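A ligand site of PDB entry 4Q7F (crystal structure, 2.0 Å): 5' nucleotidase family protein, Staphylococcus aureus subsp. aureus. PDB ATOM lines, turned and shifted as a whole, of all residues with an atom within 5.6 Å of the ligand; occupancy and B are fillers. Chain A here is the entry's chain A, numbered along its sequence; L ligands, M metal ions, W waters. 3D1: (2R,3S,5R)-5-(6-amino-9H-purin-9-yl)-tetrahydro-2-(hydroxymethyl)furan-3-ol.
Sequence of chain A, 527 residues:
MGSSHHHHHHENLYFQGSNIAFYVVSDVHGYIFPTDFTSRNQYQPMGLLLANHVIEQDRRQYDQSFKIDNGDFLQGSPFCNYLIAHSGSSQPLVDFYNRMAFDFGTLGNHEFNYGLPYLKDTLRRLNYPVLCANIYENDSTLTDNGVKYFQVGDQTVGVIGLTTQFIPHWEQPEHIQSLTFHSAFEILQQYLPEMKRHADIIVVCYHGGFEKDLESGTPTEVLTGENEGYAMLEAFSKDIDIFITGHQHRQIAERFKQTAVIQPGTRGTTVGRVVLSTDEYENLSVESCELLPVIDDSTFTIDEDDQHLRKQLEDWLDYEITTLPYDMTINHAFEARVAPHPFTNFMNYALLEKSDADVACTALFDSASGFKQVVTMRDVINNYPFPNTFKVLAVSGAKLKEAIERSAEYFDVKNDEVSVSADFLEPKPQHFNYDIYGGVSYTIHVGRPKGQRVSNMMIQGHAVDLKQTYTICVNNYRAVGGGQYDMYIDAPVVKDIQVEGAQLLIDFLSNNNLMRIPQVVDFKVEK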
ATOM      1  N   HIS A  29      17.687 -17.956 -16.597  1.00  0.00           N
ATOM      2  CA  HIS A  29      18.940 -18.016 -17.333  1.00  0.00           C
ATOM      3  C   HIS A  29      19.386 -19.385 -17.772  1.00  0.00           C
ATOM      4  O   HIS A  29      20.581 -19.671 -17.840  1.00  0.00           O
ATOM      5  CB  HIS A  29      20.052 -17.315 -16.539  1.00  0.00           C
ATOM      6  CG  HIS A  29      20.087 -15.824 -16.722  1.00  0.00           C
ATOM      7  ND1 HIS A  29      20.390 -15.238 -17.922  1.00  0.00           N
ATOM      8  CD2 HIS A  29      19.917 -14.807 -15.845  1.00  0.00           C
ATOM      9  CE1 HIS A  29      20.392 -13.926 -17.789  1.00  0.00           C
ATOM     10  NE2 HIS A  29      20.098 -13.636 -16.541  1.00  0.00           N
ATOM     11  N   ASP A  72      15.005 -13.277 -19.575  1.00  0.00           N
ATOM     12  CA  ASP A  72      16.358 -13.813 -19.392  1.00  0.00           C
ATOM     13  C   ASP A  72      16.264 -15.295 -19.131  1.00  0.00           C
ATOM     14  O   ASP A  72      16.782 -15.818 -18.137  1.00  0.00           O
ATOM     15  CB  ASP A  72      17.156 -13.085 -18.293  1.00  0.00           C
ATOM     16  CG  ASP A  72      17.821 -11.807 -18.802  1.00  0.00           C
ATOM     17  OD1 ASP A  72      17.594 -11.436 -19.983  1.00  0.00           O
ATOM     18  OD2 ASP A  72      18.568 -11.168 -18.032  1.00  0.00           O
ATOM     19  N   ASN A 109      16.899  -8.875 -21.958  1.00  0.00           N
ATOM     20  CA  ASN A 109      17.931  -8.526 -22.911  1.00  0.00           C
ATOM     21  C   ASN A 109      18.711  -9.709 -23.480  1.00  0.00           C
ATOM     22  O   ASN A 109      19.118  -9.673 -24.644  1.00  0.00           O
ATOM     23  CB  ASN A 109      18.923  -7.500 -22.313  1.00  0.00           C
ATOM     24  CG  ASN A 109      19.577  -7.985 -21.031  1.00  0.00           C
ATOM     25  OD1 ASN A 109      18.911  -8.131 -20.007  1.00  0.00           O
ATOM     26  ND2 ASN A 109      20.890  -8.170 -21.069  1.00  0.00           N
ATOM     27  N   HIS A 110      18.944 -10.729 -22.673  1.00  0.00           N
ATOM     28  CA  HIS A 110      19.693 -11.913 -23.101  1.00  0.00           C
ATOM     29  C   HIS A 110      18.968 -12.796 -24.100  1.00  0.00           C
ATOM     30  O   HIS A 110      19.575 -13.679 -24.712  1.00  0.00           O
ATOM     31  CB  HIS A 110      20.234 -12.684 -21.887  1.00  0.00           C
ATOM     32  CG  HIS A 110      21.221 -11.894 -21.093  1.00  0.00           C
ATOM     33  ND1 HIS A 110      22.517 -11.717 -21.521  1.00  0.00           N
ATOM     34  CD2 HIS A 110      21.101 -11.189 -19.946  1.00  0.00           C
ATOM     35  CE1 HIS A 110      23.173 -10.962 -20.654  1.00  0.00           C
ATOM     36  NE2 HIS A 110      22.322 -10.603 -19.705  1.00  0.00           N
ATOM     37  N   ASN A 113      20.855 -12.407 -27.337  1.00  0.00           N
ATOM     38  CA  ASN A 113      22.259 -12.832 -27.385  1.00  0.00           C
ATOM     39  C   ASN A 113      22.637 -13.782 -28.506  1.00  0.00           C
ATOM     40  O   ASN A 113      23.797 -13.834 -28.863  1.00  0.00           O
ATOM     41  CB  ASN A 113      22.677 -13.545 -26.081  1.00  0.00           C
ATOM     42  CG  ASN A 113      22.978 -12.586 -24.917  1.00  0.00           C
ATOM     43  OD1 ASN A 113      23.409 -13.051 -23.853  1.00  0.00           O
ATOM     44  ND2 ASN A 113      22.803 -11.288 -25.109  1.00  0.00           N
ATOM     45  N   TRP A 170      24.402  -2.983 -25.205  1.00  0.00           N
ATOM     46  CA  TRP A 170      25.020  -4.280 -24.910  1.00  0.00           C
ATOM     47  C   TRP A 170      25.131  -5.289 -26.051  1.00  0.00           C
ATOM     48  O   TRP A 170      26.123  -6.010 -26.171  1.00  0.00           O
ATOM     49  CB  TRP A 170      24.213  -5.008 -23.807  1.00  0.00           C
ATOM     50  CG  TRP A 170      23.906  -4.208 -22.557  1.00  0.00           C
ATOM     51  CD1 TRP A 170      24.795  -3.442 -21.831  1.00  0.00           C
ATOM     52  CD2 TRP A 170      22.661  -4.131 -21.872  1.00  0.00           C
ATOM     53  NE1 TRP A 170      24.150  -2.877 -20.751  1.00  0.00           N
ATOM     54  CE2 TRP A 170      22.836  -3.285 -20.755  1.00  0.00           C
ATOM     55  CE3 TRP A 170      21.383  -4.696 -22.099  1.00  0.00           C
ATOM     56  CZ2 TRP A 170      21.797  -2.995 -19.873  1.00  0.00           C
ATOM     57  CZ3 TRP A 170      20.373  -4.395 -21.229  1.00  0.00           C
ATOM     58  CH2 TRP A 170      20.571  -3.550 -20.142  1.00  0.00           C
ATOM     59  N   GLU A 226      18.378   2.827 -18.210  1.00  0.00           N
ATOM     60  CA  GLU A 226      18.441   1.355 -18.232  1.00  0.00           C
ATOM     61  C   GLU A 226      17.316   0.798 -17.386  1.00  0.00           C
ATOM     62  O   GLU A 226      16.587  -0.109 -17.801  1.00  0.00           O
ATOM     63  CB  GLU A 226      19.780   0.845 -17.663  1.00  0.00           C
ATOM     64  CG  GLU A 226      19.775  -0.681 -17.437  1.00  0.00           C
ATOM     65  CD  GLU A 226      21.063  -1.239 -16.840  1.00  0.00           C
ATOM     66  OE1 GLU A 226      21.092  -2.458 -16.538  1.00  0.00           O
ATOM     67  OE2 GLU A 226      22.037  -0.476 -16.659  1.00  0.00           O
ATOM     68  N   HIS A 247      15.809  -8.472 -14.081  1.00  0.00           N
ATOM     69  CA  HIS A 247      17.021  -7.888 -14.659  1.00  0.00           C
ATOM     70  C   HIS A 247      18.188  -7.625 -13.730  1.00  0.00           C
ATOM     71  O   HIS A 247      19.336  -7.883 -14.100  1.00  0.00           O
ATOM     72  CB  HIS A 247      16.680  -6.583 -15.398  1.00  0.00           C
ATOM     73  CG  HIS A 247      17.843  -5.929 -16.065  1.00  0.00           C
ATOM     74  ND1 HIS A 247      18.539  -6.524 -17.102  1.00  0.00           N
ATOM     75  CD2 HIS A 247      18.416  -4.709 -15.884  1.00  0.00           C
ATOM     76  CE1 HIS A 247      19.487  -5.714 -17.508  1.00  0.00           C
ATOM     77  NE2 HIS A 247      19.436  -4.613 -16.796  1.00  0.00           N
ATOM     78  N   HIS A 249      18.464  -9.048 -10.744  1.00  0.00           N
ATOM     79  CA  HIS A 249      18.725 -10.246  -9.940  1.00  0.00           C
ATOM     80  C   HIS A 249      18.611  -9.988  -8.434  1.00  0.00           C
ATOM     81  O   HIS A 249      19.222 -10.680  -7.611  1.00  0.00           O
ATOM     82  CB  HIS A 249      20.091 -10.817 -10.249  1.00  0.00           C
ATOM     83  CG  HIS A 249      20.297 -11.187 -11.678  1.00  0.00           C
ATOM     84  ND1 HIS A 249      21.399 -11.878 -12.108  1.00  0.00           N
ATOM     85  CD2 HIS A 249      19.488 -11.051 -12.758  1.00  0.00           C
ATOM     86  CE1 HIS A 249      21.295 -12.089 -13.414  1.00  0.00           C
ATOM     87  NE2 HIS A 249      20.136 -11.641 -13.818  1.00  0.00           N
ATOM     88  N   PHE A 365      35.179 -12.560 -14.968  1.00  0.00           N
ATOM     89  CA  PHE A 365      33.768 -12.871 -14.678  1.00  0.00           C
ATOM     90  C   PHE A 365      33.557 -13.594 -13.321  1.00  0.00           C
ATOM     91  O   PHE A 365      34.458 -14.234 -12.781  1.00  0.00           O
ATOM     92  CB  PHE A 365      33.119 -13.583 -15.885  1.00  0.00           C
ATOM     93  CG  PHE A 365      33.172 -12.755 -17.150  1.00  0.00           C
ATOM     94  CD1 PHE A 365      32.399 -11.596 -17.272  1.00  0.00           C
ATOM     95  CD2 PHE A 365      33.973 -13.118 -18.226  1.00  0.00           C
ATOM     96  CE1 PHE A 365      32.447 -10.821 -18.426  1.00  0.00           C
ATOM     97  CE2 PHE A 365      34.021 -12.343 -19.380  1.00  0.00           C
ATOM     98  CZ  PHE A 365      33.261 -11.197 -19.488  1.00  0.00           C
ATOM     99  N   TYR A 384      34.582 -17.866 -19.215  1.00  0.00           N
ATOM    100  CA  TYR A 384      34.025 -16.927 -20.216  1.00  0.00           C
ATOM    101  C   TYR A 384      32.573 -17.332 -20.432  1.00  0.00           C
ATOM    102  O   TYR A 384      32.282 -18.002 -21.418  1.00  0.00           O
ATOM    103  CB  TYR A 384      34.790 -16.945 -21.565  1.00  0.00           C
ATOM    104  CG  TYR A 384      34.693 -15.585 -22.185  1.00  0.00           C
ATOM    105  CD1 TYR A 384      33.520 -15.147 -22.766  1.00  0.00           C
ATOM    106  CD2 TYR A 384      35.745 -14.685 -22.053  1.00  0.00           C
ATOM    107  CE1 TYR A 384      33.417 -13.868 -23.268  1.00  0.00           C
ATOM    108  CE2 TYR A 384      35.643 -13.392 -22.558  1.00  0.00           C
ATOM    109  CZ  TYR A 384      34.482 -13.001 -23.148  1.00  0.00           C
ATOM    110  OH  TYR A 384      34.342 -11.722 -23.630  1.00  0.00           O
ATOM    111  N   PHE A 386      29.859 -15.591 -21.325  1.00  0.00           N
ATOM    112  CA  PHE A 386      29.006 -14.852 -22.237  1.00  0.00           C
ATOM    113  C   PHE A 386      29.351 -15.170 -23.685  1.00  0.00           C
ATOM    114  O   PHE A 386      30.498 -15.488 -23.997  1.00  0.00           O
ATOM    115  CB  PHE A 386      29.113 -13.358 -21.980  1.00  0.00           C
ATOM    116  CG  PHE A 386      28.580 -12.950 -20.638  1.00  0.00           C
ATOM    117  CD1 PHE A 386      27.211 -12.933 -20.394  1.00  0.00           C
ATOM    118  CD2 PHE A 386      29.438 -12.575 -19.629  1.00  0.00           C
ATOM    119  CE1 PHE A 386      26.712 -12.567 -19.162  1.00  0.00           C
ATOM    120  CE2 PHE A 386      28.944 -12.193 -18.387  1.00  0.00           C
ATOM    121  CZ  PHE A 386      27.590 -12.181 -18.162  1.00  0.00           C
ATOM    122  N   PRO A 387      28.359 -15.054 -24.594  1.00  0.00           N
ATOM    123  CA  PRO A 387      28.666 -15.293 -25.993  1.00  0.00           C
ATOM    124  C   PRO A 387      29.171 -14.019 -26.714  1.00  0.00           C
ATOM    125  O   PRO A 387      28.592 -13.564 -27.704  1.00  0.00           O
ATOM    126  CB  PRO A 387      27.348 -15.821 -26.541  1.00  0.00           C
ATOM    127  CG  PRO A 387      26.294 -15.161 -25.702  1.00  0.00           C
ATOM    128  CD  PRO A 387      26.919 -14.833 -24.368  1.00  0.00           C
ATOM    129  N   ASN A 388      30.252 -13.440 -26.204  1.00  0.00           N
ATOM    130  CA  ASN A 388      30.850 -12.255 -26.785  1.00  0.00           C
ATOM    131  C   ASN A 388      31.848 -12.548 -27.904  1.00  0.00           C
ATOM    132  O   ASN A 388      32.606 -13.510 -27.819  1.00  0.00           O
ATOM    133  CB  ASN A 388      31.697 -11.515 -25.773  1.00  0.00           C
ATOM    134  CG  ASN A 388      30.943 -11.062 -24.550  1.00  0.00           C
ATOM    135  OD1 ASN A 388      31.531 -11.004 -23.451  1.00  0.00           O
ATOM    136  ND2 ASN A 388      29.689 -10.708 -24.705  1.00  0.00           N
ATOM    137  N   PHE A 432      32.052  -7.613 -13.196  1.00  0.00           N
ATOM    138  CA  PHE A 432      32.255  -7.779 -14.622  1.00  0.00           C
ATOM    139  C   PHE A 432      32.457  -6.444 -15.360  1.00  0.00           C
ATOM    140  O   PHE A 432      32.700  -6.443 -16.561  1.00  0.00           O
ATOM    141  CB  PHE A 432      31.101  -8.573 -15.237  1.00  0.00           C
ATOM    142  CG  PHE A 432      29.727  -8.084 -14.847  1.00  0.00           C
ATOM    143  CD1 PHE A 432      29.240  -6.869 -15.298  1.00  0.00           C
ATOM    144  CD2 PHE A 432      28.884  -8.886 -14.067  1.00  0.00           C
ATOM    145  CE1 PHE A 432      27.973  -6.426 -14.950  1.00  0.00           C
ATOM    146  CE2 PHE A 432      27.603  -8.458 -13.726  1.00  0.00           C
ATOM    147  CZ  PHE A 432      27.139  -7.224 -14.180  1.00  0.00           C
ATOM    148  N   ASN A 433      32.346  -5.323 -14.646  1.00  0.00           N
ATOM    149  CA  ASN A 433      32.573  -4.010 -15.221  1.00  0.00           C
ATOM    150  C   ASN A 433      33.968  -3.498 -14.932  1.00  0.00           C
ATOM    151  O   ASN A 433      34.231  -2.344 -15.181  1.00  0.00           O
ATOM    152  CB  ASN A 433      31.512  -2.998 -14.804  1.00  0.00           C
ATOM    153  CG  ASN A 433      30.209  -3.189 -15.558  1.00  0.00           C
ATOM    154  OD1 ASN A 433      30.158  -3.876 -16.582  1.00  0.00           O
ATOM    155  ND2 ASN A 433      29.150  -2.578 -15.056  1.00  0.00           N
ATOM    156  N   ASN A 475      35.744  -6.723 -26.034  1.00  0.00           N
ATOM    157  CA  ASN A 475      34.612  -7.607 -26.432  1.00  0.00           C
ATOM    158  C   ASN A 475      33.454  -6.803 -27.026  1.00  0.00           C
ATOM    159  O   ASN A 475      33.434  -5.569 -26.893  1.00  0.00           O
ATOM    160  CB  ASN A 475      34.188  -8.523 -25.304  1.00  0.00           C
ATOM    161  CG  ASN A 475      33.589  -7.783 -24.118  1.00  0.00           C
ATOM    162  OD1 ASN A 475      32.771  -6.883 -24.268  1.00  0.00           O
ATOM    163  ND2 ASN A 475      33.920  -8.235 -22.939  1.00  0.00           N
ATOM    164  N   TYR A 477      30.452  -6.411 -26.121  1.00  0.00           N
ATOM    165  CA  TYR A 477      29.678  -5.747 -25.058  1.00  0.00           C
ATOM    166  C   TYR A 477      30.319  -4.389 -24.822  1.00  0.00           C
ATOM    167  O   TYR A 477      29.656  -3.358 -24.870  1.00  0.00           O
ATOM    168  CB  TYR A 477      29.723  -6.592 -23.775  1.00  0.00           C
ATOM    169  CG  TYR A 477      28.912  -6.107 -22.616  1.00  0.00           C
ATOM    170  CD1 TYR A 477      27.550  -6.387 -22.524  1.00  0.00           C
ATOM    171  CD2 TYR A 477      29.512  -5.426 -21.554  1.00  0.00           C
ATOM    172  CE1 TYR A 477      26.798  -5.963 -21.455  1.00  0.00           C
ATOM    173  CE2 TYR A 477      28.777  -5.011 -20.458  1.00  0.00           C
ATOM    174  CZ  TYR A 477      27.411  -5.282 -20.420  1.00  0.00           C
ATOM    175  OH  TYR A 477      26.666  -4.900 -19.345  1.00  0.00           O
ATOM    176  N   ARG A 478      31.620  -4.408 -24.564  1.00  0.00           N
ATOM    177  CA  ARG A 478      32.346  -3.155 -24.381  1.00  0.00           C
ATOM    178  C   ARG A 478      32.278  -2.228 -25.604  1.00  0.00           C
ATOM    179  O   ARG A 478      32.140  -1.015 -25.434  1.00  0.00           O
ATOM    180  CB  ARG A 478      33.792  -3.435 -24.048  1.00  0.00           C
ATOM    181  CG  ARG A 478      34.011  -3.941 -22.660  1.00  0.00           C
ATOM    182  CD  ARG A 478      33.883  -2.844 -21.616  1.00  0.00           C
ATOM    183  NE  ARG A 478      34.243  -3.423 -20.321  1.00  0.00           N
ATOM    184  CZ  ARG A 478      33.388  -3.931 -19.439  1.00  0.00           C
ATOM    185  NH1 ARG A 478      32.070  -3.906 -19.617  1.00  0.00           N
ATOM    186  NH2 ARG A 478      33.885  -4.463 -18.337  1.00  0.00           N
HETATM  187  O5' 3D1 L   1      23.230  -4.684 -17.229  1.00  0.00           O
HETATM  188  C5' 3D1 L   1      24.184  -5.471 -17.924  1.00  0.00           C
HETATM  189  C4' 3D1 L   1      23.584  -6.803 -18.346  1.00  0.00           C
HETATM  190  O4' 3D1 L   1      24.501  -7.390 -19.253  1.00  0.00           O
HETATM  191  C1' 3D1 L   1      25.119  -8.562 -18.704  1.00  0.00           C
HETATM  192  N9  3D1 L   1      26.574  -8.551 -19.021  1.00  0.00           N
HETATM  193  C4  3D1 L   1      27.031  -9.026 -20.171  1.00  0.00           C
HETATM  194  N3  3D1 L   1      26.442  -9.575 -21.256  1.00  0.00           N
HETATM  195  C2  3D1 L   1      27.191  -9.968 -22.316  1.00  0.00           C
HETATM  196  N1  3D1 L   1      28.540  -9.826 -22.351  1.00  0.00           N
HETATM  197  C6  3D1 L   1      29.245  -9.286 -21.333  1.00  0.00           C
HETATM  198  N6  3D1 L   1      30.599  -9.155 -21.413  1.00  0.00           N
HETATM  199  C5  3D1 L   1      28.493  -8.826 -20.142  1.00  0.00           C
HETATM  200  N7  3D1 L   1      28.780  -8.253 -18.952  1.00  0.00           N
HETATM  201  C8  3D1 L   1      27.615  -8.085 -18.283  1.00  0.00           C
HETATM  202  C2' 3D1 L   1      24.746  -8.591 -17.225  1.00  0.00           C
HETATM  203  C3' 3D1 L   1      23.430  -7.838 -17.246  1.00  0.00           C
HETATM  204  O3' 3D1 L   1      22.384  -8.772 -17.586  1.00  0.00           O
HETATM  205 MG    MG M   1      18.485  -8.895 -17.922  1.00  0.00          MG
HETATM  206 MN    MN M   2      19.430 -11.529 -16.062  1.00  0.00          MN
HETATM  207  O   HOH W   1      30.886  -6.608 -18.472  1.00  0.00           O
HETATM  208  O   HOH W   2      21.648  -6.270 -14.725  1.00  0.00           O
HETATM  209  O   HOH W   3      21.781 -11.214 -16.624  1.00  0.00           O
HETATM  210  O   HOH W   4      23.978  -9.110 -23.302  1.00  0.00           O
HETATM  211  O   HOH W   5      20.061  -9.368 -16.290  1.00  0.00           O
HETATM  212  O   HOH W   6      32.833  -7.403 -20.534  1.00  0.00           O
HETATM  213  O   HOH W   7      26.272  -8.607 -25.132  1.00  0.00           O
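Water W3 lies within hydrogen-bond range of an oxygen (O3') of the ligand (2.7 Å) and a ring nitrogen (NE2) of His 110 (3.2 Å). Water W5 lies within hydrogen-bond range of an oxygen (O3') of the ligand (2.7 Å) and the backbone carbonyl oxygen of His 247 (2.7 Å). Water W6 lies within hydrogen-bond range of ND2 of Asn 475 (2.8 Å) and N6 of the ligand (3.0 Å). Water W4 lies within hydrogen-bond range of ND2 of Asn 113 (3.1 Å), N3 of the ligand (3.2 Å) and ND1 of His 110 (3.5 Å). Water W2 bridges the backbone carbonyl oxygen (O) of His 247 (2.9 Å) and an oxygen (O5') of the ligand (3.4 Å).
An oxygen (O4') of the ligand lies close to the side-chain hydroxyl (OH) of Tyr 477 (3.3 Å). O3' of the ligand sits at hydrogen-bond distance from NE2 of His 110, 2.8 Å away. OE1 of Glu 226 is in hydrogen-bond range of O5' of the ligand, at 3.2 Å. A nitrogen (N1) of the ligand lies within hydrogen-bond range of the side-chain amide nitrogen (ND2) of Asn 388 (2.8 Å).
The side-chain amide oxygen (OD1) of Asn 388 sits at hydrogen-bond distance from the side-chain hydroxyl (OH) of Tyr 384. A ring nitrogen (ND1) of His 110 sits at hydrogen-bond distance from the side-chain amide oxygen (OD1) of Asn 113 (2.8 Å). A ring nitrogen (NE2) of His 247 is in hydrogen-bond range of the side-chain carboxylate (OE1) of Glu 226, at 2.7 Å. OD1 of Asp 72 lies within hydrogen-bond range of N of His 110 (3.1 Å). The side-chain amide oxygen (OD1) of Asn 475 lies within hydrogen-bond range of the backbone NH (N) of Tyr 477 (3.0 Å). A ring nitrogen (NE2) of His 110 is in hydrogen-bond range of the side-chain amide nitrogen (ND2) of Asn 109, 3.1 Å away. The backbone carbonyl oxygen of Phe 432 is in hydrogen-bond range of the guanidinium group of Arg 478, 2.9 Å away. OD1 of Asn 475 is in hydrogen-bond range of N of Arg 478.
Residues that only touch the ligand: Asn 109 (3.8 Å), Trp 170 (3.4 Å), His 247 (3.8 Å), Phe 365 (3.9 Å), Phe 386 (3.5 Å), Phe 432 (3.6 Å) and Asn 475 (3.8 Å). Hydrophobic or aromatic side chains that line the ligand: His 110, Trp 170, His 247, Phe 365, Phe 386, Phe 432 and Tyr 477. Within 4 Å of the ligand: Asn 109, His 110, Trp 170, Glu 226, His 247, Phe 365, Phe 386, Asn 388, Phe 432, Asn 475 and Tyr 477.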
